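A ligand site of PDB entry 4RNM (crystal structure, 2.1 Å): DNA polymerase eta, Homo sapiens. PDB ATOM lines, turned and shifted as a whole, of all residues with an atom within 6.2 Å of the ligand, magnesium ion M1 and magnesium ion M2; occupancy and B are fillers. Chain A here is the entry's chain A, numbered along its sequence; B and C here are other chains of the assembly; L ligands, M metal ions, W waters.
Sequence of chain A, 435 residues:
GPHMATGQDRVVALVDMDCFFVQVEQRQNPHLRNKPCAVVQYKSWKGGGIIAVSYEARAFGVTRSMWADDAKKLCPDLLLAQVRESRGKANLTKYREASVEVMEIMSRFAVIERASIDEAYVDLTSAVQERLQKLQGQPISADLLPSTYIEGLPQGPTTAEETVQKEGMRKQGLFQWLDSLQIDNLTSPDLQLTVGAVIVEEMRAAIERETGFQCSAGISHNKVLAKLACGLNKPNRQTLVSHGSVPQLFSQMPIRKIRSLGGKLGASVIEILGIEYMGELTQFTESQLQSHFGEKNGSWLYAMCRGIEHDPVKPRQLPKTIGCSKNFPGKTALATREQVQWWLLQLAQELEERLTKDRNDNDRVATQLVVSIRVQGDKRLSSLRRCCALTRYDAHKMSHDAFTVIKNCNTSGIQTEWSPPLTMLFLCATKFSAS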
ATOM      1  N   ASP A  16       7.319   0.579 -26.887  1.00  0.00           N
ATOM      2  CA  ASP A  16       8.509  -0.223 -26.680  1.00  0.00           C
ATOM      3  C   ASP A  16       8.248  -1.440 -25.768  1.00  0.00           C
ATOM      4  O   ASP A  16       7.757  -1.289 -24.654  1.00  0.00           O
ATOM      5  CB  ASP A  16       9.593   0.651 -26.091  1.00  0.00           C
ATOM      6  CG  ASP A  16      10.937  -0.029 -26.082  1.00  0.00           C
ATOM      7  OD1 ASP A  16      11.721   0.175 -27.052  1.00  0.00           O
ATOM      8  OD2 ASP A  16      11.203  -0.767 -25.119  1.00  0.00           O
ATOM      9  N   MET A  17       8.596  -2.628 -26.242  1.00  0.00           N
ATOM     10  CA  MET A  17       8.385  -3.845 -25.463  1.00  0.00           C
ATOM     11  C   MET A  17       9.221  -3.849 -24.184  1.00  0.00           C
ATOM     12  O   MET A  17      10.396  -3.476 -24.185  1.00  0.00           O
ATOM     13  CB  MET A  17       8.705  -5.089 -26.297  1.00  0.00           C
ATOM     14  CG  MET A  17       8.049  -5.119 -27.680  1.00  0.00           C
ATOM     15  SD  MET A  17       6.255  -4.928 -27.664  1.00  0.00           S
ATOM     16  CE  MET A  17       5.782  -6.170 -26.476  1.00  0.00           C
ATOM     17  N   ASP A  18       8.587  -4.230 -23.088  1.00  0.00           N
ATOM     18  CA  ASP A  18       9.288  -4.350 -21.817  1.00  0.00           C
ATOM     19  C   ASP A  18      10.192  -5.570 -21.863  1.00  0.00           C
ATOM     20  O   ASP A  18       9.750  -6.609 -22.322  1.00  0.00           O
ATOM     21  CB  ASP A  18       8.284  -4.446 -20.663  1.00  0.00           C
ATOM     22  CG  ASP A  18       7.447  -3.192 -20.506  1.00  0.00           C
ATOM     23  OD1 ASP A  18       7.918  -2.127 -20.901  1.00  0.00           O
ATOM     24  OD2 ASP A  18       6.312  -3.281 -19.987  1.00  0.00           O
ATOM     25  N   CYS A  19      11.442  -5.399 -21.403  1.00  0.00           N
ATOM     26  CA  CYS A  19      12.494  -6.421 -21.418  1.00  0.00           C
ATOM     27  C   CYS A  19      12.217  -7.524 -22.468  1.00  0.00           C
ATOM     28  O   CYS A  19      11.938  -8.670 -22.136  1.00  0.00           O
ATOM     29  CB  CYS A  19      12.672  -7.029 -20.013  1.00  0.00           C
ATOM     30  SG  CYS A  19      11.189  -7.754 -19.211  1.00  0.00           S
ATOM     31  N   PHE A  20      12.266  -7.120 -23.736  1.00  0.00           N
ATOM     32  CA  PHE A  20      11.649  -7.874 -24.835  1.00  0.00           C
ATOM     33  C   PHE A  20      12.155  -9.329 -24.982  1.00  0.00           C
ATOM     34  O   PHE A  20      11.338 -10.251 -24.964  1.00  0.00           O
ATOM     35  CB  PHE A  20      11.848  -7.087 -26.137  1.00  0.00           C
ATOM     36  CG  PHE A  20      11.185  -7.723 -27.331  1.00  0.00           C
ATOM     37  CD1 PHE A  20       9.878  -8.163 -27.254  1.00  0.00           C
ATOM     38  CD2 PHE A  20      11.875  -7.895 -28.513  1.00  0.00           C
ATOM     39  CE1 PHE A  20       9.259  -8.760 -28.316  1.00  0.00           C
ATOM     40  CE2 PHE A  20      11.254  -8.485 -29.607  1.00  0.00           C
ATOM     41  CZ  PHE A  20       9.946  -8.923 -29.508  1.00  0.00           C
ATOM     42  N   PHE A  21      13.460  -9.543 -25.112  1.00  0.00           N
ATOM     43  CA  PHE A  21      13.982 -10.915 -25.305  1.00  0.00           C
ATOM     44  C   PHE A  21      13.633 -11.786 -24.105  1.00  0.00           C
ATOM     45  O   PHE A  21      13.347 -12.964 -24.265  1.00  0.00           O
ATOM     46  CB  PHE A  21      15.497 -10.942 -25.531  1.00  0.00           C
ATOM     47  CG  PHE A  21      15.948 -10.403 -26.871  1.00  0.00           C
ATOM     48  CD1 PHE A  21      15.122  -9.606 -27.644  1.00  0.00           C
ATOM     49  CD2 PHE A  21      17.230 -10.660 -27.330  1.00  0.00           C
ATOM     50  CE1 PHE A  21      15.556  -9.092 -28.865  1.00  0.00           C
ATOM     51  CE2 PHE A  21      17.672 -10.158 -28.554  1.00  0.00           C
ATOM     52  CZ  PHE A  21      16.840  -9.369 -29.313  1.00  0.00           C
ATOM     53  N   VAL A  22      13.635 -11.199 -22.901  1.00  0.00           N
ATOM     54  CA  VAL A  22      13.223 -11.921 -21.702  1.00  0.00           C
ATOM     55  C   VAL A  22      11.750 -12.369 -21.790  1.00  0.00           C
ATOM     56  O   VAL A  22      11.450 -13.532 -21.547  1.00  0.00           O
ATOM     57  CB  VAL A  22      13.422 -11.058 -20.438  1.00  0.00           C
ATOM     58  CG1 VAL A  22      12.737 -11.685 -19.238  1.00  0.00           C
ATOM     59  CG2 VAL A  22      14.917 -10.866 -20.158  1.00  0.00           C
ATOM     60  N   GLN A  41      24.170 -14.247 -24.279  1.00  0.00           N
ATOM     61  CA  GLN A  41      24.716 -14.646 -25.570  1.00  0.00           C
ATOM     62  C   GLN A  41      26.022 -15.377 -25.332  1.00  0.00           C
ATOM     63  O   GLN A  41      26.909 -14.845 -24.656  1.00  0.00           O
ATOM     64  CB  GLN A  41      24.937 -13.424 -26.475  1.00  0.00           C
ATOM     65  CG  GLN A  41      24.337 -13.550 -27.846  1.00  0.00           C
ATOM     66  CD  GLN A  41      24.254 -12.211 -28.583  1.00  0.00           C
ATOM     67  OE1 GLN A  41      25.046 -11.298 -28.335  1.00  0.00           O
ATOM     68  NE2 GLN A  41      23.295 -12.091 -29.491  1.00  0.00           N
ATOM     69  N   ILE A  51      22.182  -9.602 -22.651  1.00  0.00           N
ATOM     70  CA  ILE A  51      21.655  -8.570 -23.541  1.00  0.00           C
ATOM     71  C   ILE A  51      20.212  -8.157 -23.226  1.00  0.00           C
ATOM     72  O   ILE A  51      19.674  -7.237 -23.852  1.00  0.00           O
ATOM     73  CB  ILE A  51      21.749  -8.994 -25.009  1.00  0.00           C
ATOM     74  CG1 ILE A  51      20.858 -10.193 -25.295  1.00  0.00           C
ATOM     75  CG2 ILE A  51      23.218  -9.315 -25.374  1.00  0.00           C
ATOM     76  CD1 ILE A  51      20.892 -10.589 -26.757  1.00  0.00           C
ATOM     77  N   ALA A  52      19.592  -8.806 -22.243  1.00  0.00           N
ATOM     78  CA  ALA A  52      18.260  -8.400 -21.779  1.00  0.00           C
ATOM     79  C   ALA A  52      18.009  -8.894 -20.358  1.00  0.00           C
ATOM     80  O   ALA A  52      18.416  -9.989 -20.004  1.00  0.00           O
ATOM     81  CB  ALA A  52      17.169  -8.915 -22.715  1.00  0.00           C
ATOM     82  N   VAL A  53      17.307  -8.084 -19.567  1.00  0.00           N
ATOM     83  CA  VAL A  53      17.200  -8.310 -18.127  1.00  0.00           C
ATOM     84  C   VAL A  53      15.779  -8.084 -17.646  1.00  0.00           C
ATOM     85  O   VAL A  53      15.225  -6.993 -17.832  1.00  0.00           O
ATOM     86  CB  VAL A  53      18.137  -7.355 -17.330  1.00  0.00           C
ATOM     87  CG1 VAL A  53      18.096  -7.696 -15.848  1.00  0.00           C
ATOM     88  CG2 VAL A  53      19.566  -7.414 -17.857  1.00  0.00           C
ATOM     89  N   TYR A  55      12.780  -7.214 -15.055  1.00  0.00           N
ATOM     90  CA  TYR A  55      12.728  -6.193 -14.014  1.00  0.00           C
ATOM     91  C   TYR A  55      12.958  -6.748 -12.613  1.00  0.00           C
ATOM     92  O   TYR A  55      13.404  -6.027 -11.732  1.00  0.00           O
ATOM     93  CB  TYR A  55      11.400  -5.441 -14.089  1.00  0.00           C
ATOM     94  CG  TYR A  55      11.423  -4.454 -15.243  1.00  0.00           C
ATOM     95  CD1 TYR A  55      11.223  -4.876 -16.552  1.00  0.00           C
ATOM     96  CD2 TYR A  55      11.699  -3.106 -15.022  1.00  0.00           C
ATOM     97  CE1 TYR A  55      11.279  -3.995 -17.617  1.00  0.00           C
ATOM     98  CE2 TYR A  55      11.741  -2.195 -16.104  1.00  0.00           C
ATOM     99  CZ  TYR A  55      11.532  -2.654 -17.395  1.00  0.00           C
ATOM    100  OH  TYR A  55      11.570  -1.783 -18.473  1.00  0.00           O
ATOM    101  N   ARG A  58      16.650  -6.700 -12.505  1.00  0.00           N
ATOM    102  CA  ARG A  58      17.194  -5.326 -12.487  1.00  0.00           C
ATOM    103  C   ARG A  58      17.233  -4.781 -11.066  1.00  0.00           C
ATOM    104  O   ARG A  58      18.122  -3.999 -10.702  1.00  0.00           O
ATOM    105  CB  ARG A  58      16.382  -4.382 -13.384  1.00  0.00           C
ATOM    106  CG  ARG A  58      16.429  -4.711 -14.868  1.00  0.00           C
ATOM    107  CD  ARG A  58      15.603  -3.748 -15.704  1.00  0.00           C
ATOM    108  NE  ARG A  58      15.331  -4.323 -17.016  1.00  0.00           N
ATOM    109  CZ  ARG A  58      14.945  -3.644 -18.097  1.00  0.00           C
ATOM    110  NH1 ARG A  58      14.791  -2.333 -18.050  1.00  0.00           N
ATOM    111  NH2 ARG A  58      14.730  -4.288 -19.233  1.00  0.00           N
ATOM    112  N   ARG A  64      22.441  -4.993 -18.730  1.00  0.00           N
ATOM    113  CA  ARG A  64      22.892  -5.375 -20.066  1.00  0.00           C
ATOM    114  C   ARG A  64      24.396  -5.198 -20.198  1.00  0.00           C
ATOM    115  O   ARG A  64      24.976  -4.283 -19.610  1.00  0.00           O
ATOM    116  CB  ARG A  64      22.158  -4.538 -21.116  1.00  0.00           C
ATOM    117  CG  ARG A  64      22.649  -4.722 -22.536  1.00  0.00           C
ATOM    118  CD  ARG A  64      21.724  -4.082 -23.564  1.00  0.00           C
ATOM    119  NE  ARG A  64      21.440  -2.664 -23.330  1.00  0.00           N
ATOM    120  CZ  ARG A  64      20.298  -2.208 -22.836  1.00  0.00           C
ATOM    121  NH1 ARG A  64      19.331  -3.065 -22.487  1.00  0.00           N
ATOM    122  NH2 ARG A  64      20.101  -0.908 -22.658  1.00  0.00           N
ATOM    123  N   SER A 116      13.254  -0.256 -34.061  1.00  0.00           N
ATOM    124  CA  SER A 116      14.193  -1.272 -33.594  1.00  0.00           C
ATOM    125  C   SER A 116      13.457  -2.593 -33.614  1.00  0.00           C
ATOM    126  O   SER A 116      12.263  -2.623 -33.931  1.00  0.00           O
ATOM    127  CB  SER A 116      14.700  -0.958 -32.179  1.00  0.00           C
ATOM    128  OG  SER A 116      13.702  -1.257 -31.205  1.00  0.00           O
ATOM    129  N   ILE A 117      14.131  -3.668 -33.242  1.00  0.00           N
ATOM    130  CA  ILE A 117      13.470  -4.966 -33.155  1.00  0.00           C
ATOM    131  C   ILE A 117      12.285  -4.938 -32.177  1.00  0.00           C
ATOM    132  O   ILE A 117      11.373  -5.763 -32.308  1.00  0.00           O
ATOM    133  CB  ILE A 117      14.474  -6.086 -32.724  1.00  0.00           C
ATOM    134  CG1 ILE A 117      13.935  -7.471 -33.119  1.00  0.00           C
ATOM    135  CG2 ILE A 117      14.775  -6.012 -31.234  1.00  0.00           C
ATOM    136  CD1 ILE A 117      14.977  -8.596 -32.970  1.00  0.00           C
ATOM    137  N   ASP A 118      12.261  -4.010 -31.210  1.00  0.00           N
ATOM    138  CA  ASP A 118      11.202  -4.044 -30.200  1.00  0.00           C
ATOM    139  C   ASP A 118      10.415  -2.744 -30.024  1.00  0.00           C
ATOM    140  O   ASP A 118       9.683  -2.577 -29.032  1.00  0.00           O
ATOM    141  CB  ASP A 118      11.775  -4.494 -28.842  1.00  0.00           C
ATOM    142  CG  ASP A 118      12.185  -3.312 -27.946  1.00  0.00           C
ATOM    143  OD1 ASP A 118      12.838  -2.373 -28.452  1.00  0.00           O
ATOM    144  OD2 ASP A 118      11.863  -3.334 -26.737  1.00  0.00           O
ATOM    145  N   GLU A 119      10.534  -1.827 -30.966  1.00  0.00           N
ATOM    146  CA  GLU A 119       9.749  -0.604 -30.853  1.00  0.00           C
ATOM    147  C   GLU A 119       9.375   0.004 -32.201  1.00  0.00           C
ATOM    148  O   GLU A 119      10.041  -0.196 -33.205  1.00  0.00           O
ATOM    149  CB  GLU A 119      10.492   0.441 -30.005  1.00  0.00           C
ATOM    150  CG  GLU A 119      11.656   1.107 -30.678  1.00  0.00           C
ATOM    151  CD  GLU A 119      12.751   1.477 -29.682  1.00  0.00           C
ATOM    152  OE1 GLU A 119      12.869   2.675 -29.335  1.00  0.00           O
ATOM    153  OE2 GLU A 119      13.468   0.567 -29.227  1.00  0.00           O
ATOM    154  N   SER A 216       5.530  -0.720 -22.847  1.00  0.00           N
ATOM    155  CA  SER A 216       5.236   0.637 -22.439  1.00  0.00           C
ATOM    156  C   SER A 216       5.063   1.496 -23.683  1.00  0.00           C
ATOM    157  O   SER A 216       5.404   1.072 -24.779  1.00  0.00           O
ATOM    158  CB  SER A 216       6.359   1.173 -21.564  1.00  0.00           C
ATOM    159  OG  SER A 216       6.582   0.289 -20.496  1.00  0.00           O
ATOM    160  N   LYS A 227       9.231   9.074 -27.498  1.00  0.00           N
ATOM    161  CA  LYS A 227      10.283   8.177 -27.022  1.00  0.00           C
ATOM    162  C   LYS A 227      10.670   8.482 -25.551  1.00  0.00           C
ATOM    163  O   LYS A 227      10.730   7.592 -24.716  1.00  0.00           O
ATOM    164  CB  LYS A 227      11.507   8.270 -27.958  1.00  0.00           C
ATOM    165  CG  LYS A 227      12.741   7.488 -27.518  1.00  0.00           C
ATOM    166  CD  LYS A 227      12.443   6.001 -27.270  1.00  0.00           C
ATOM    167  CE  LYS A 227      13.713   5.211 -26.868  1.00  0.00           C
ATOM    168  NZ  LYS A 227      13.492   3.707 -26.787  1.00  0.00           N
ATOM    169  N   LYS A 234       7.982   3.057 -17.504  1.00  0.00           N
ATOM    170  CA  LYS A 234       8.220   1.634 -17.739  1.00  0.00           C
ATOM    171  C   LYS A 234       8.380   0.918 -16.408  1.00  0.00           C
ATOM    172  O   LYS A 234       8.958   1.474 -15.491  1.00  0.00           O
ATOM    173  CB  LYS A 234       9.479   1.400 -18.575  1.00  0.00           C
ATOM    174  CG  LYS A 234       9.400   1.894 -19.987  1.00  0.00           C
ATOM    175  CD  LYS A 234      10.544   1.327 -20.852  1.00  0.00           C
ATOM    176  CE  LYS A 234      10.387  -0.156 -21.055  1.00  0.00           C
ATOM    177  NZ  LYS A 234      10.021  -0.636 -22.438  1.00  0.00           N
ATOM    178  N   PRO A 235       7.924  -0.352 -16.296  1.00  0.00           N
ATOM    179  CA  PRO A 235       7.305  -1.207 -17.311  1.00  0.00           C
ATOM    180  C   PRO A 235       5.770  -1.243 -17.227  1.00  0.00           C
ATOM    181  O   PRO A 235       5.207  -0.852 -16.214  1.00  0.00           O
ATOM    182  CB  PRO A 235       7.878  -2.578 -16.976  1.00  0.00           C
ATOM    183  CG  PRO A 235       7.914  -2.560 -15.460  1.00  0.00           C
ATOM    184  CD  PRO A 235       8.271  -1.125 -15.093  1.00  0.00           C
ATOM    185  P    DT B   8      18.296   3.808 -27.726  1.00  0.00           P
ATOM    186  OP1  DT B   8      17.181   4.486 -27.035  1.00  0.00           O
ATOM    187  OP2  DT B   8      19.579   3.533 -27.049  1.00  0.00           O
ATOM    188  O5'  DT B   8      17.893   2.351 -28.259  1.00  0.00           O
ATOM    189  C5'  DT B   8      16.980   2.153 -29.337  1.00  0.00           C
ATOM    190  C4'  DT B   8      16.824   0.668 -29.562  1.00  0.00           C
ATOM    191  O4'  DT B   8      18.030   0.139 -30.182  1.00  0.00           O
ATOM    192  C3'  DT B   8      16.611  -0.118 -28.265  1.00  0.00           C
ATOM    193  O3'  DT B   8      15.563  -1.081 -28.424  1.00  0.00           O
ATOM    194  C2'  DT B   8      17.979  -0.784 -28.014  1.00  0.00           C
ATOM    195  C1'  DT B   8      18.550  -0.926 -29.418  1.00  0.00           C
ATOM    196  N1   DT B   8      20.044  -0.849 -29.463  1.00  0.00           N
ATOM    197  C2   DT B   8      20.748  -1.829 -30.136  1.00  0.00           C
ATOM    198  O2   DT B   8      20.229  -2.760 -30.708  1.00  0.00           O
ATOM    199  N3   DT B   8      22.110  -1.671 -30.135  1.00  0.00           N
ATOM    200  C4   DT B   8      22.821  -0.669 -29.534  1.00  0.00           C
ATOM    201  O4   DT B   8      24.036  -0.619 -29.570  1.00  0.00           O
ATOM    202  C5   DT B   8      22.037   0.334 -28.826  1.00  0.00           C
ATOM    203  C7   DT B   8      22.737   1.469 -28.128  1.00  0.00           C
ATOM    204  C6   DT B   8      20.700   0.193 -28.828  1.00  0.00           C
ATOM    205  O5' 3DR C   4      29.622  -7.120 -29.039  1.00  0.00           O
ATOM    206  P   3DR C   4      29.812  -5.608 -28.334  1.00  0.00           P
ATOM    207  OP1 3DR C   4      31.098  -5.011 -28.762  1.00  0.00           O
ATOM    208  OP2 3DR C   4      28.686  -4.727 -28.675  1.00  0.00           O
ATOM    209  C2' 3DR C   4      27.201  -8.840 -29.119  1.00  0.00           C
ATOM    210  C5' 3DR C   4      30.057  -8.272 -28.331  1.00  0.00           C
ATOM    211  C4' 3DR C   4      29.371  -9.529 -28.732  1.00  0.00           C
ATOM    212  O4' 3DR C   4      28.374 -10.034 -27.504  1.00  0.00           O
ATOM    213  C1' 3DR C   4      27.358  -9.196 -27.563  1.00  0.00           C
ATOM    214  C3' 3DR C   4      28.516  -9.404 -29.754  1.00  0.00           C
ATOM    215  O3' 3DR C   4      28.261 -10.729 -30.306  1.00  0.00           O
ATOM    216  P    DA C   5      28.374 -10.996 -31.890  1.00  0.00           P
ATOM    217  OP1  DA C   5      28.406 -12.469 -32.071  1.00  0.00           O
ATOM    218  OP2  DA C   5      29.483 -10.191 -32.467  1.00  0.00           O
ATOM    219  O5'  DA C   5      26.962 -10.509 -32.441  1.00  0.00           O
ATOM    220  C5'  DA C   5      25.779 -11.107 -31.907  1.00  0.00           C
ATOM    221  C4'  DA C   5      24.537 -10.605 -32.604  1.00  0.00           C
ATOM    222  O4'  DA C   5      24.201  -9.274 -32.109  1.00  0.00           O
ATOM    223  C3'  DA C   5      24.625 -10.486 -34.118  1.00  0.00           C
ATOM    224  O3'  DA C   5      23.358 -10.798 -34.685  1.00  0.00           O
ATOM    225  C2'  DA C   5      25.014  -9.014 -34.309  1.00  0.00           C
ATOM    226  C1'  DA C   5      24.240  -8.351 -33.179  1.00  0.00           C
ATOM    227  N9   DA C   5      24.851  -7.114 -32.666  1.00  0.00           N
ATOM    228  C8   DA C   5      26.185  -6.863 -32.492  1.00  0.00           C
ATOM    229  N7   DA C   5      26.427  -5.673 -31.993  1.00  0.00           N
ATOM    230  C5   DA C   5      25.175  -5.117 -31.828  1.00  0.00           C
ATOM    231  C6   DA C   5      24.743  -3.864 -31.318  1.00  0.00           C
ATOM    232  N6   DA C   5      25.567  -2.915 -30.888  1.00  0.00           N
ATOM    233  N1   DA C   5      23.411  -3.636 -31.275  1.00  0.00           N
ATOM    234  C2   DA C   5      22.577  -4.593 -31.700  1.00  0.00           C
ATOM    235  N3   DA C   5      22.865  -5.797 -32.201  1.00  0.00           N
ATOM    236  C4   DA C   5      24.189  -6.002 -32.219  1.00  0.00           C
HETATM  237  N1  LIG L   1      23.158  -5.316 -28.092  1.00  0.00           N
HETATM  238  C1  LIG L   1      22.551  -6.484 -28.423  1.00  0.00           C
HETATM  239  N2  LIG L   1      21.188  -6.632 -28.236  1.00  0.00           N
HETATM  240  C2  LIG L   1      20.473  -5.607 -27.727  1.00  0.00           C
HETATM  241  C3  LIG L   1      21.086  -4.461 -27.397  1.00  0.00           C
HETATM  242  C4  LIG L   1      22.450  -4.303 -27.585  1.00  0.00           C
HETATM  243  N3  LIG L   1      23.249  -3.165 -27.308  1.00  0.00           N
HETATM  244  N4  LIG L   1      20.163  -3.597 -26.915  1.00  0.00           N
HETATM  245  C5  LIG L   1      18.963  -4.221 -26.923  1.00  0.00           C
HETATM  246  N5  LIG L   1      19.139  -5.461 -27.414  1.00  0.00           N
HETATM  247  P1  LIG L   1      15.566  -2.367 -25.336  1.00  0.00           P
HETATM  248  P2  LIG L   1      14.443  -4.096 -23.291  1.00  0.00           P
HETATM  249  P3  LIG L   1      13.136  -2.241 -21.679  1.00  0.00           P
HETATM  250  C6  LIG L   1      18.108  -6.386 -27.573  1.00  0.00           C
HETATM  251  O1  LIG L   1      14.186  -1.881 -25.671  1.00  0.00           O
HETATM  252  O2  LIG L   1      13.280  -4.202 -24.270  1.00  0.00           O
HETATM  253  O3  LIG L   1      11.938  -2.615 -20.873  1.00  0.00           O
HETATM  254  C7  LIG L   1      17.739  -6.986 -26.422  1.00  0.00           C
HETATM  255  O4  LIG L   1      16.574  -1.290 -25.384  1.00  0.00           O
HETATM  256  O5  LIG L   1      15.099  -5.447 -23.050  1.00  0.00           O
HETATM  257  O6  LIG L   1      14.038  -1.327 -20.920  1.00  0.00           O
HETATM  258  C8  LIG L   1      16.478  -6.232 -25.932  1.00  0.00           C
HETATM  259  O7  LIG L   1      15.574  -6.994 -25.286  1.00  0.00           O
HETATM  260  N6  LIG L   1      15.561  -3.014 -23.832  1.00  0.00           N
HETATM  261  O8  LIG L   1      14.004  -3.558 -21.914  1.00  0.00           O
HETATM  262  O9  LIG L   1      12.724  -1.678 -23.018  1.00  0.00           O
HETATM  263  C9  LIG L   1      15.850  -5.671 -27.259  1.00  0.00           C
HETATM  264  O10 LIG L   1      16.855  -5.487 -28.076  1.00  0.00           O
HETATM  265  C10 LIG L   1      15.124  -4.359 -27.002  1.00  0.00           C
HETATM  266  O11 LIG L   1      16.034  -3.434 -26.424  1.00  0.00           O
HETATM  267 MG    MG M   1      12.268  -2.498 -24.838  1.00  0.00          MG
HETATM  268 MG    MG M   2      13.528  -0.604 -27.528  1.00  0.00          MG
HETATM  269  O   HOH W   1      26.024  -3.438 -27.630  1.00  0.00           O
HETATM  270  O   HOH W   2      18.650  -5.282 -30.981  1.00  0.00           O
HETATM  271  O   HOH W   3      16.412  -5.744 -20.951  1.00  0.00           O
HETATM  272  O   HOH W   4      13.565   1.034 -19.400  1.00  0.00           O
HETATM  273  O   HOH W   5      13.591   0.738 -23.589  1.00  0.00           O
HETATM  274  O   HOH W   6      25.757  -6.197 -27.959  1.00  0.00           O
HETATM  275  O   HOH W   7      14.404   0.767 -26.240  1.00  0.00           O
HETATM  276  O   HOH W   8      16.349  -3.236 -29.746  1.00  0.00           O
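Magnesium ion M2 is bound by OD1 of Asp 16, OE2 of Glu 119, water W7, OD1 of Asp 118, O3' of DT 8 of chain B and O1 of the ligand. Magnesium ion M2 has six donor atoms within binding distance.
NH1 of Arg 58 is in salt-bridge range of O6 of the ligand (3.1 Å). An oxygen (O3) of the ligand sits at hydrogen-bond distance from the side-chain hydroxyl (OH) of Tyr 55 (2.6 Å). NZ of Lys 234 lies within salt-bridge range of O3 of the ligand, 3.2 Å away. The backbone NH of Phe 21 lies within hydrogen-bond range of an oxygen (O7) of the ligand. A nitrogen (N3) of the ligand lies close to N3 of DT 8 of chain B (3.4 Å). N of Cys 19 sits at hydrogen-bond distance from O3 of the ligand, 2.9 Å away. O5 of the ligand is in hydrogen-bond range of N of Phe 20, at 3.4 Å.
Magnesium ion M1 is bound by an oxygen (O9) of the ligand (2.0 Å), the side-chain carboxylate of Asp 16 (2.1 Å), an oxygen (O2) of the ligand (2.1 Å), the side-chain carboxylate of Asp 118 (2.1 Å), an oxygen (O1) of the ligand (2.2 Å) and the backbone carbonyl oxygen of Met 17 (2.2 Å). Magnesium ion M1 has six donor atoms within binding distance.
Water W7 bridges O4 of the ligand (3.1 Å) and NZ of Lys 227 (3.1 Å). Water W3 lies within hydrogen-bond range of O5 of the ligand (2.5 Å), NH2 of Arg 58 (2.8 Å) and N of Val 53 (2.9 Å). Water W6 lies within hydrogen-bond range of N1 of the ligand (2.7 Å) and OP2 of 3DR 4 of chain C (3.4 Å). Water W1 lies within hydrogen-bond range of a nitrogen (N3) of the ligand (2.8 Å), OP2 of 3DR 4 of chain C (3.1 Å) and N6 of DA 5 of chain C (3.3 Å). Water W2 lies within hydrogen-bond range of O2 of DT 8 of chain B and O10 of the ligand.
NZ of Lys 234 touches magnesium ion M1, at 3.8 Å. Within 4 Å of magnesium ion M1: Asp 16, Met 17, Asp 118 and Lys 234.
OG of Ser 116 touches magnesium ion M2 (3.7 Å). Of the 25 residues printed, 5 come within 4 Å of magnesium ion M2. Along chain A the residues within 4 Å of magnesium ion M2 span positions 16 to 119. The nearest printed residue that does not touch magnesium ion M2 is Lys 227 (4.4 Å).
The guanidinium group (NE) of Arg 58 lies within hydrogen-bond range of the backbone carbonyl oxygen (O) of Val 53. The side-chain carboxylate of Asp 16 lies close to the side-chain amino group of Lys 227 (3.96 Å). The backbone carbonyl oxygen of Met 17 sits close to the side-chain amino group of Lys 234 (3.4 Å). The side-chain amino group of Lys 227 is in salt-bridge range of the side-chain carboxylate of Glu 119, 2.8 Å away. The side-chain hydroxyl (OH) of Tyr 55 is in hydrogen-bond range of the guanidinium group (NH1) of Arg 58. O3' of DT 8 of chain B lies close to the side-chain hydroxyl of Ser 116, 3.4 Å away. The backbone carbonyl oxygen (O) of Asp 16 sits at hydrogen-bond distance from the side-chain amino group (NZ) of Lys 234 (3.2 Å). OD1 of Asp 18 lies within hydrogen-bond range of OG of Ser 216, at 2.8 Å.
Residues that only touch the ligand: Ile 51 (3.2 Å), Asp 18 (3.3 Å), Ala 52 (3.6 Å), DA 5 of chain C (3.6 Å), Arg 64 (3.7 Å) and Ile 117 (3.8 Å). Hydrophobic or aromatic side chains within 4 Å of the ligand: Phe 20, Phe 21, Ala 52, Tyr 55 and Ile 117. 16 residues have an atom within 4 Å of the ligand: Asp 16, Met 17, Asp 18, Cys 19, Phe 20, Phe 21, Ile 51, Ala 52, Tyr 55, Arg 58, Arg 64, Ile 117, Asp 118, Lys 234, DT 8 of chain B and DA 5 of chain C. The nearest printed residue that does not touch the ligand is Glu 119 (4.4 Å).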
